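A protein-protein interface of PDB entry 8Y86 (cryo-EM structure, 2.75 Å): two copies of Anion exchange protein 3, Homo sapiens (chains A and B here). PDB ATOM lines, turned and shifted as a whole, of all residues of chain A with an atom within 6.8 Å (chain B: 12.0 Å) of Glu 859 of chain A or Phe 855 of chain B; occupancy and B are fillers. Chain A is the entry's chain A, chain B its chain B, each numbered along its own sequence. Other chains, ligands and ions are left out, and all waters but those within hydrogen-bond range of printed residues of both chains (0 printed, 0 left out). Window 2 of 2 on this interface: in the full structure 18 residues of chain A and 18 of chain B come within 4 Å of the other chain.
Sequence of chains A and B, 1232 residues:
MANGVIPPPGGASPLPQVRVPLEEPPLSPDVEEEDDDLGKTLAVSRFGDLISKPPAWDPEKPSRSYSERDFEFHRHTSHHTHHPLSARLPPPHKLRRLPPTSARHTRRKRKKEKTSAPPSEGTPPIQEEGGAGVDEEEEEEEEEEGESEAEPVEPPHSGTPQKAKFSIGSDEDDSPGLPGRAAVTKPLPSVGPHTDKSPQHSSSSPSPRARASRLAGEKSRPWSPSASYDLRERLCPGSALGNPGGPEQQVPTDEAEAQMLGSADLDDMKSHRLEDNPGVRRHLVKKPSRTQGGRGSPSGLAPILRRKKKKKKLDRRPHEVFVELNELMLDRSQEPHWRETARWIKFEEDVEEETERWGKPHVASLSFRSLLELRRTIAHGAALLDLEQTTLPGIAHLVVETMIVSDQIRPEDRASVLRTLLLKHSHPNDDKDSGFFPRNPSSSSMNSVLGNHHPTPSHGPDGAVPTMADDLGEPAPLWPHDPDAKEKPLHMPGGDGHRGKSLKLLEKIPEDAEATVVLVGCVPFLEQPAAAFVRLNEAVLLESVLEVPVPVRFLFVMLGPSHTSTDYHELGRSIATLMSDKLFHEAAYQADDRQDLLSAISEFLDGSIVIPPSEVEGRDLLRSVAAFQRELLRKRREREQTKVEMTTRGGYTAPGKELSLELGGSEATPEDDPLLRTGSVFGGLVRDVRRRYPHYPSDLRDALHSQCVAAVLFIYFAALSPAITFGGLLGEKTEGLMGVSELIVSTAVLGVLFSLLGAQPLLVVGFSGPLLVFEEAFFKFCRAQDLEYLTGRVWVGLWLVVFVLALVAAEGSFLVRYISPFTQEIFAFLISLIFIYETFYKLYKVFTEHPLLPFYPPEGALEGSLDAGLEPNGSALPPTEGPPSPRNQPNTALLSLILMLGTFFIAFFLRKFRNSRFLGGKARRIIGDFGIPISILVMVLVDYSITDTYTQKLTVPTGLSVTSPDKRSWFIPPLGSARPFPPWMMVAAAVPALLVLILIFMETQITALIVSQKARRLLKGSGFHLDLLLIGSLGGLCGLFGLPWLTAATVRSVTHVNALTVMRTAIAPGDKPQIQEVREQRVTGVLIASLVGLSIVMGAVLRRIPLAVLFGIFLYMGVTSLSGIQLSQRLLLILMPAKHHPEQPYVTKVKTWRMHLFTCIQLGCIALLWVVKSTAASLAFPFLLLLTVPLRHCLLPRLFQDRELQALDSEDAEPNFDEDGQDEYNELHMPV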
ATOM      1  N   TYR A 856      -0.967  14.052  -7.185  1.00  0.00           N
ATOM      2  CA  TYR A 856      -2.326  13.727  -6.756  1.00  0.00           C
ATOM      3  C   TYR A 856      -2.758  14.754  -5.718  1.00  0.00           C
ATOM      4  O   TYR A 856      -2.527  14.570  -4.513  1.00  0.00           O
ATOM      5  CB  TYR A 856      -2.399  12.308  -6.198  1.00  0.00           C
ATOM      6  CG  TYR A 856      -2.407  11.242  -7.268  1.00  0.00           C
ATOM      7  CD1 TYR A 856      -3.510  11.065  -8.090  1.00  0.00           C
ATOM      8  CD2 TYR A 856      -1.308  10.418  -7.463  1.00  0.00           C
ATOM      9  CE1 TYR A 856      -3.519  10.095  -9.070  1.00  0.00           C
ATOM     10  CE2 TYR A 856      -1.310   9.447  -8.442  1.00  0.00           C
ATOM     11  CZ  TYR A 856      -2.417   9.290  -9.243  1.00  0.00           C
ATOM     12  OH  TYR A 856      -2.423   8.322 -10.218  1.00  0.00           O
ATOM     13  N   PRO A 857      -3.390  15.853  -6.138  1.00  0.00           N
ATOM     14  CA  PRO A 857      -3.739  16.899  -5.181  1.00  0.00           C
ATOM     15  C   PRO A 857      -4.886  16.459  -4.289  1.00  0.00           C
ATOM     16  O   PRO A 857      -5.757  15.679  -4.711  1.00  0.00           O
ATOM     17  CB  PRO A 857      -4.146  18.083  -6.078  1.00  0.00           C
ATOM     18  CG  PRO A 857      -4.265  17.541  -7.477  1.00  0.00           C
ATOM     19  CD  PRO A 857      -3.990  16.074  -7.463  1.00  0.00           C
ATOM     20  N   PRO A 858      -4.926  16.932  -3.046  1.00  0.00           N
ATOM     21  CA  PRO A 858      -6.009  16.538  -2.139  1.00  0.00           C
ATOM     22  C   PRO A 858      -7.353  17.090  -2.591  1.00  0.00           C
ATOM     23  O   PRO A 858      -7.446  18.123  -3.258  1.00  0.00           O
ATOM     24  CB  PRO A 858      -5.585  17.144  -0.796  1.00  0.00           C
ATOM     25  CG  PRO A 858      -4.710  18.295  -1.170  1.00  0.00           C
ATOM     26  CD  PRO A 858      -3.980  17.864  -2.410  1.00  0.00           C
ATOM     27  N   GLU A 859      -8.406  16.372  -2.213  1.00  0.00           N
ATOM     28  CA  GLU A 859      -9.769  16.759  -2.556  1.00  0.00           C
ATOM     29  C   GLU A 859     -10.157  18.072  -1.882  1.00  0.00           C
ATOM     30  O   GLU A 859     -10.434  19.066  -2.553  1.00  0.00           O
ATOM     31  CB  GLU A 859     -10.753  15.655  -2.159  1.00  0.00           C
ATOM     32  CG  GLU A 859     -10.523  14.331  -2.870  1.00  0.00           C
ATOM     33  CD  GLU A 859     -10.842  14.400  -4.351  1.00  0.00           C
ATOM     34  OE1 GLU A 859     -11.777  15.139  -4.726  1.00  0.00           O
ATOM     35  OE2 GLU A 859     -10.157  13.716  -5.141  1.00  0.00           O
ATOM     36  N   ARG A 887     -12.867   9.261  -7.858  1.00  0.00           N
ATOM     37  CA  ARG A 887     -12.174   9.306  -9.136  1.00  0.00           C
ATOM     38  C   ARG A 887     -10.772   9.857  -8.927  1.00  0.00           C
ATOM     39  O   ARG A 887     -10.524  10.616  -7.986  1.00  0.00           O
ATOM     40  CB  ARG A 887     -12.929  10.163 -10.158  1.00  0.00           C
ATOM     41  CG  ARG A 887     -13.683   9.366 -11.203  1.00  0.00           C
ATOM     42  CD  ARG A 887     -14.178  10.264 -12.323  1.00  0.00           C
ATOM     43  NE  ARG A 887     -14.399   9.528 -13.562  1.00  0.00           N
ATOM     44  CZ  ARG A 887     -13.651   9.652 -14.649  1.00  0.00           C
ATOM     45  NH1 ARG A 887     -12.614  10.472 -14.685  1.00  0.00           N
ATOM     46  NH2 ARG A 887     -13.950   8.935 -15.728  1.00  0.00           N
ATOM     47  N   ASN A 888      -9.860   9.467  -9.818  1.00  0.00           N
ATOM     48  CA  ASN A 888      -8.465   9.908  -9.786  1.00  0.00           C
ATOM     49  C   ASN A 888      -7.812   9.567  -8.445  1.00  0.00           C
ATOM     50  O   ASN A 888      -7.367  10.440  -7.697  1.00  0.00           O
ATOM     51  CB  ASN A 888      -8.359  11.407 -10.087  1.00  0.00           C
ATOM     52  CG  ASN A 888      -8.729  11.744 -11.515  1.00  0.00           C
ATOM     53  OD1 ASN A 888      -8.336  11.049 -12.450  1.00  0.00           O
ATOM     54  ND2 ASN A 888      -9.489  12.815 -11.691  1.00  0.00           N
ATOM     55  N   GLN A 889      -7.757   8.268  -8.155  1.00  0.00           N
ATOM     56  CA  GLN A 889      -7.195   7.787  -6.904  1.00  0.00           C
ATOM     57  C   GLN A 889      -5.856   7.102  -7.143  1.00  0.00           C
ATOM     58  O   GLN A 889      -5.658   6.480  -8.194  1.00  0.00           O
ATOM     59  CB  GLN A 889      -8.148   6.805  -6.215  1.00  0.00           C
ATOM     60  CG  GLN A 889      -9.477   7.414  -5.813  1.00  0.00           C
ATOM     61  CD  GLN A 889      -9.355   8.351  -4.632  1.00  0.00           C
ATOM     62  OE1 GLN A 889      -8.570   8.114  -3.716  1.00  0.00           O
ATOM     63  NE2 GLN A 889     -10.127   9.429  -4.651  1.00  0.00           N
ATOM     64  N   PRO A 890      -4.920   7.201  -6.204  1.00  0.00           N
ATOM     65  CA  PRO A 890      -3.632   6.525  -6.369  1.00  0.00           C
ATOM     66  C   PRO A 890      -3.683   5.068  -5.939  1.00  0.00           C
ATOM     67  O   PRO A 890      -4.495   4.665  -5.103  1.00  0.00           O
ATOM     68  CB  PRO A 890      -2.699   7.330  -5.459  1.00  0.00           C
ATOM     69  CG  PRO A 890      -3.594   7.846  -4.394  1.00  0.00           C
ATOM     70  CD  PRO A 890      -4.924   8.108  -5.042  1.00  0.00           C
ATOM     71  N   ASP A 948      -5.418   1.530   3.122  1.00  0.00           N
ATOM     72  CA  ASP A 948      -5.155   2.922   2.783  1.00  0.00           C
ATOM     73  C   ASP A 948      -5.723   3.186   1.396  1.00  0.00           C
ATOM     74  O   ASP A 948      -6.002   4.330   1.028  1.00  0.00           O
ATOM     75  CB  ASP A 948      -3.658   3.240   2.830  1.00  0.00           C
ATOM     76  CG  ASP A 948      -2.998   2.765   4.110  1.00  0.00           C
ATOM     77  OD1 ASP A 948      -2.702   1.556   4.216  1.00  0.00           O
ATOM     78  OD2 ASP A 948      -2.780   3.602   5.012  1.00  0.00           O
ATOM     79  N   GLU B 849      10.413   2.185   1.394  1.00  0.00           N
ATOM     80  CA  GLU B 849      10.822   3.538   1.024  1.00  0.00           C
ATOM     81  C   GLU B 849       9.660   4.357   0.472  1.00  0.00           C
ATOM     82  O   GLU B 849       9.587   5.567   0.716  1.00  0.00           O
ATOM     83  CB  GLU B 849      11.960   3.482   0.008  1.00  0.00           C
ATOM     84  CG  GLU B 849      13.332   3.707   0.609  1.00  0.00           C
ATOM     85  CD  GLU B 849      14.436   3.069  -0.208  1.00  0.00           C
ATOM     86  OE1 GLU B 849      15.535   2.851   0.344  1.00  0.00           O
ATOM     87  OE2 GLU B 849      14.206   2.785  -1.403  1.00  0.00           O
ATOM     88  N   HIS B 850       8.744   3.725  -0.264  1.00  0.00           N
ATOM     89  CA  HIS B 850       7.632   4.403  -0.928  1.00  0.00           C
ATOM     90  C   HIS B 850       6.329   3.746  -0.493  1.00  0.00           C
ATOM     91  O   HIS B 850       5.754   2.931  -1.228  1.00  0.00           O
ATOM     92  CB  HIS B 850       7.784   4.354  -2.448  1.00  0.00           C
ATOM     93  CG  HIS B 850       9.024   5.020  -2.955  1.00  0.00           C
ATOM     94  ND1 HIS B 850       9.251   6.372  -2.821  1.00  0.00           N
ATOM     95  CD2 HIS B 850      10.107   4.520  -3.594  1.00  0.00           C
ATOM     96  CE1 HIS B 850      10.418   6.676  -3.358  1.00  0.00           C
ATOM     97  NE2 HIS B 850      10.959   5.570  -3.833  1.00  0.00           N
ATOM     98  N   PRO B 851       5.832   4.081   0.694  1.00  0.00           N
ATOM     99  CA  PRO B 851       4.654   3.390   1.226  1.00  0.00           C
ATOM    100  C   PRO B 851       3.372   3.810   0.523  1.00  0.00           C
ATOM    101  O   PRO B 851       3.309   4.818  -0.183  1.00  0.00           O
ATOM    102  CB  PRO B 851       4.639   3.812   2.697  1.00  0.00           C
ATOM    103  CG  PRO B 851       5.296   5.144   2.698  1.00  0.00           C
ATOM    104  CD  PRO B 851       6.348   5.094   1.628  1.00  0.00           C
ATOM    105  N   LEU B 852       2.331   3.005   0.733  1.00  0.00           N
ATOM    106  CA  LEU B 852       1.004   3.276   0.190  1.00  0.00           C
ATOM    107  C   LEU B 852       0.254   4.170   1.172  1.00  0.00           C
ATOM    108  O   LEU B 852      -0.180   3.711   2.232  1.00  0.00           O
ATOM    109  CB  LEU B 852       0.243   1.977  -0.060  1.00  0.00           C
ATOM    110  CG  LEU B 852       0.894   0.916  -0.950  1.00  0.00           C
ATOM    111  CD1 LEU B 852      -0.147  -0.066  -1.450  1.00  0.00           C
ATOM    112  CD2 LEU B 852       1.622   1.554  -2.119  1.00  0.00           C
ATOM    113  N   LEU B 853       0.098   5.443   0.816  1.00  0.00           N
ATOM    114  CA  LEU B 853      -0.517   6.420   1.697  1.00  0.00           C
ATOM    115  C   LEU B 853      -1.895   6.827   1.183  1.00  0.00           C
ATOM    116  O   LEU B 853      -2.171   6.728  -0.016  1.00  0.00           O
ATOM    117  CB  LEU B 853       0.360   7.671   1.824  1.00  0.00           C
ATOM    118  CG  LEU B 853       1.744   7.489   2.444  1.00  0.00           C
ATOM    119  CD1 LEU B 853       2.539   8.777   2.354  1.00  0.00           C
ATOM    120  CD2 LEU B 853       1.626   7.029   3.884  1.00  0.00           C
ATOM    121  N   PRO B 854      -2.787   7.282   2.069  1.00  0.00           N
ATOM    122  CA  PRO B 854      -4.089   7.780   1.592  1.00  0.00           C
ATOM    123  C   PRO B 854      -3.972   9.038   0.749  1.00  0.00           C
ATOM    124  O   PRO B 854      -4.580   9.123  -0.325  1.00  0.00           O
ATOM    125  CB  PRO B 854      -4.860   8.030   2.896  1.00  0.00           C
ATOM    126  CG  PRO B 854      -4.170   7.189   3.919  1.00  0.00           C
ATOM    127  CD  PRO B 854      -2.727   7.230   3.539  1.00  0.00           C
ATOM    128  N   PHE B 855      -3.206  10.022   1.210  1.00  0.00           N
ATOM    129  CA  PHE B 855      -3.025  11.286   0.512  1.00  0.00           C
ATOM    130  C   PHE B 855      -1.550  11.493   0.201  1.00  0.00           C
ATOM    131  O   PHE B 855      -0.680  11.107   0.988  1.00  0.00           O
ATOM    132  CB  PHE B 855      -3.551  12.459   1.343  1.00  0.00           C
ATOM    133  CG  PHE B 855      -5.030  12.680   1.212  1.00  0.00           C
ATOM    134  CD1 PHE B 855      -5.570  13.137   0.022  1.00  0.00           C
ATOM    135  CD2 PHE B 855      -5.879  12.430   2.275  1.00  0.00           C
ATOM    136  CE1 PHE B 855      -6.930  13.341  -0.104  1.00  0.00           C
ATOM    137  CE2 PHE B 855      -7.241  12.633   2.155  1.00  0.00           C
ATOM    138  CZ  PHE B 855      -7.766  13.088   0.964  1.00  0.00           C
ATOM    139  N   TYR B 856      -1.275  12.111  -0.947  1.00  0.00           N
ATOM    140  CA  TYR B 856       0.087  12.357  -1.421  1.00  0.00           C
ATOM    141  C   TYR B 856       0.231  13.843  -1.719  1.00  0.00           C
ATOM    142  O   TYR B 856       0.096  14.271  -2.875  1.00  0.00           O
ATOM    143  CB  TYR B 856       0.398  11.513  -2.654  1.00  0.00           C
ATOM    144  CG  TYR B 856       0.710  10.069  -2.336  1.00  0.00           C
ATOM    145  CD1 TYR B 856       1.886   9.719  -1.690  1.00  0.00           C
ATOM    146  CD2 TYR B 856      -0.174   9.057  -2.677  1.00  0.00           C
ATOM    147  CE1 TYR B 856       2.173   8.403  -1.396  1.00  0.00           C
ATOM    148  CE2 TYR B 856       0.104   7.738  -2.386  1.00  0.00           C
ATOM    149  CZ  TYR B 856       1.279   7.417  -1.746  1.00  0.00           C
ATOM    150  OH  TYR B 856       1.562   6.104  -1.454  1.00  0.00           O
ATOM    151  N   PRO B 857       0.511  14.664  -0.712  1.00  0.00           N
ATOM    152  CA  PRO B 857       0.556  16.112  -0.924  1.00  0.00           C
ATOM    153  C   PRO B 857       1.858  16.530  -1.578  1.00  0.00           C
ATOM    154  O   PRO B 857       2.934  16.020  -1.230  1.00  0.00           O
ATOM    155  CB  PRO B 857       0.434  16.687   0.498  1.00  0.00           C
ATOM    156  CG  PRO B 857       0.661  15.529   1.444  1.00  0.00           C
ATOM    157  CD  PRO B 857       0.926  14.287   0.649  1.00  0.00           C
ATOM    158  N   PRO B 858       1.803  17.454  -2.535  1.00  0.00           N
ATOM    159  CA  PRO B 858       3.036  17.938  -3.163  1.00  0.00           C
ATOM    160  C   PRO B 858       3.882  18.744  -2.191  1.00  0.00           C
ATOM    161  O   PRO B 858       3.374  19.380  -1.264  1.00  0.00           O
ATOM    162  CB  PRO B 858       2.526  18.814  -4.313  1.00  0.00           C
ATOM    163  CG  PRO B 858       1.172  19.256  -3.869  1.00  0.00           C
ATOM    164  CD  PRO B 858       0.604  18.107  -3.085  1.00  0.00           C
ATOM    165  N   GLU B 859       5.191  18.711  -2.417  1.00  0.00           N
ATOM    166  CA  GLU B 859       6.131  19.434  -1.569  1.00  0.00           C
ATOM    167  C   GLU B 859       6.694  20.655  -2.292  1.00  0.00           C
ATOM    168  O   GLU B 859       7.813  21.088  -2.018  1.00  0.00           O
ATOM    169  CB  GLU B 859       7.270  18.514  -1.125  1.00  0.00           C
ATOM    170  CG  GLU B 859       6.821  17.342  -0.267  1.00  0.00           C
ATOM    171  CD  GLU B 859       6.306  17.776   1.090  1.00  0.00           C
ATOM    172  OE1 GLU B 859       6.817  18.782   1.628  1.00  0.00           O
ATOM    173  OE2 GLU B 859       5.391  17.113   1.620  1.00  0.00           O
ATOM    174  N   ARG B 887      11.291  10.343  -2.208  1.00  0.00           N
ATOM    175  CA  ARG B 887      10.654   9.468  -1.237  1.00  0.00           C
ATOM    176  C   ARG B 887       9.160   9.749  -1.211  1.00  0.00           C
ATOM    177  O   ARG B 887       8.703  10.825  -1.604  1.00  0.00           O
ATOM    178  CB  ARG B 887      11.245   9.644   0.167  1.00  0.00           C
ATOM    179  CG  ARG B 887      12.640   9.073   0.338  1.00  0.00           C
ATOM    180  CD  ARG B 887      13.176   9.358   1.730  1.00  0.00           C
ATOM    181  NE  ARG B 887      12.413   8.663   2.759  1.00  0.00           N
ATOM    182  CZ  ARG B 887      12.756   7.494   3.285  1.00  0.00           C
ATOM    183  NH1 ARG B 887      13.851   6.859   2.902  1.00  0.00           N
ATOM    184  NH2 ARG B 887      11.979   6.951   4.219  1.00  0.00           N
ATOM    185  N   ASN B 888       8.403   8.758  -0.736  1.00  0.00           N
ATOM    186  CA  ASN B 888       6.948   8.854  -0.609  1.00  0.00           C
ATOM    187  C   ASN B 888       6.295   9.178  -1.952  1.00  0.00           C
ATOM    188  O   ASN B 888       5.511  10.119  -2.079  1.00  0.00           O
ATOM    189  CB  ASN B 888       6.556   9.884   0.453  1.00  0.00           C
ATOM    190  CG  ASN B 888       6.980   9.472   1.847  1.00  0.00           C
ATOM    191  OD1 ASN B 888       6.838   8.315   2.236  1.00  0.00           O
ATOM    192  ND2 ASN B 888       7.507  10.422   2.607  1.00  0.00           N
ATOM    193  N   GLN B 889       6.629   8.382  -2.965  1.00  0.00           N
ATOM    194  CA  GLN B 889       6.088   8.558  -4.304  1.00  0.00           C
ATOM    195  C   GLN B 889       4.941   7.588  -4.554  1.00  0.00           C
ATOM    196  O   GLN B 889       4.959   6.462  -4.045  1.00  0.00           O
ATOM    197  CB  GLN B 889       7.171   8.336  -5.359  1.00  0.00           C
ATOM    198  CG  GLN B 889       8.353   9.281  -5.254  1.00  0.00           C
ATOM    199  CD  GLN B 889       7.990  10.709  -5.596  1.00  0.00           C
ATOM    200  OE1 GLN B 889       7.918  11.078  -6.766  1.00  0.00           O
ATOM    201  NE2 GLN B 889       7.764  11.524  -4.574  1.00  0.00           N
ATOM    202  N   PRO B 890       3.935   7.991  -5.323  1.00  0.00           N
ATOM    203  CA  PRO B 890       2.839   7.075  -5.645  1.00  0.00           C
ATOM    204  C   PRO B 890       3.175   6.162  -6.813  1.00  0.00           C
ATOM    205  O   PRO B 890       3.989   6.487  -7.680  1.00  0.00           O
ATOM    206  CB  PRO B 890       1.689   8.022  -6.006  1.00  0.00           C
ATOM    207  CG  PRO B 890       2.369   9.231  -6.531  1.00  0.00           C
ATOM    208  CD  PRO B 890       3.651   9.369  -5.763  1.00  0.00           C
ATOM    209  N   ASN B 891       2.532   4.993  -6.812  1.00  0.00           N
ATOM    210  CA  ASN B 891       2.577   4.028  -7.911  1.00  0.00           C
ATOM    211  C   ASN B 891       3.971   3.449  -8.141  1.00  0.00           C
ATOM    212  O   ASN B 891       4.226   2.854  -9.190  1.00  0.00           O
ATOM    213  CB  ASN B 891       2.051   4.642  -9.214  1.00  0.00           C
ATOM    214  CG  ASN B 891       0.708   5.317  -9.044  1.00  0.00           C
ATOM    215  OD1 ASN B 891      -0.168   4.814  -8.345  1.00  0.00           O
ATOM    216  ND2 ASN B 891       0.537   6.464  -9.686  1.00  0.00           N
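Hydrophobic or aromatic side chains of chain B within 4 Å of the printed part of chain A: Pro 854, Phe 855 and Pro 890.
Printed residues of chain A that touch a printed residue of chain B: Tyr 856, Pro 858, Glu 859 and Asp 948.
Hydrophobic or aromatic side chains of chain A within 4 Å of the printed part of chain B: Tyr 856.
Among the printed residues, no Asp or Glu carboxylate lies within 4 Å of a Lys or Arg side-chain nitrogen of the other chain.
Among the printed residues, pairs that only touch across the chains: Asp 948 of chain A with Leu 852 of chain B (3.5 Å), Tyr 856 of chain A with Asn 891 of chain B (3.5 Å), Pro 858 of chain A with Phe 855 of chain B (3.9 Å), Asp 948 of chain A with Pro 854 of chain B (3.9 Å), Tyr 856 of chain A with Pro 890 of chain B (3.97 Å) and Glu 859 of chain A with Phe 855 of chain B (3.98 Å).
Tyr 856 of chain A touches its own counterpart, Tyr 856 of chain B.
Tyr 856 of chain A touches Pro 890 of chain B, but with the chains exchanged Pro 890 of chain A does not touch Tyr 856 of chain B (4.01 Å).
Of the 7 pairs that touch across the chains among the printed residues, 1 has its exchanged pair printed and touching as well.
Of chain B, only Phe 855 comes within 4 Å of Glu 859 of chain A.
Of chain A, only Pro 858 and Glu 859 come within 4 Å of Phe 855 of chain B.
Printed residues of chain A within 4 Å of Tyr 856 of chain B: Tyr 856 (3.1 Å).
Of the printed residues of chain A, Leu 852 of chain B touches Asp 948 (3.5 Å).
Of the printed residues of chain A, Pro 890 of chain B touches Tyr 856.
Of the printed residues of chain A, Asn 891 of chain B touches Tyr 856 (3.5 Å).
Of the printed residues of chain B, Tyr 856 of chain A touches Tyr 856, Pro 890 and Asn 891.
Asn 888 of chain B touches none of the printed residues of chain A.
The nearest residue of chain A that does not touch Phe 855 of chain B is Pro 857 of chain A (5.3 Å).
The nearest printed residue of chain A that does not touch Pro 854 of chain B is Pro 890 of chain A (4.4 Å).
OH of Tyr 856 of chain B sits at hydrogen-bond distance from O of Pro 851 of chain B (2.5 Å).
The backbone NH (N) of Leu 853 of chain B lies within hydrogen-bond range of the side-chain hydroxyl (OH) of Tyr 856 of chain B (2.8 Å).
The backbone carbonyl oxygen of Tyr 856 of chain B lies close to the backbone carbonyl oxygen of Tyr 856 of chain A (3.1 Å).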
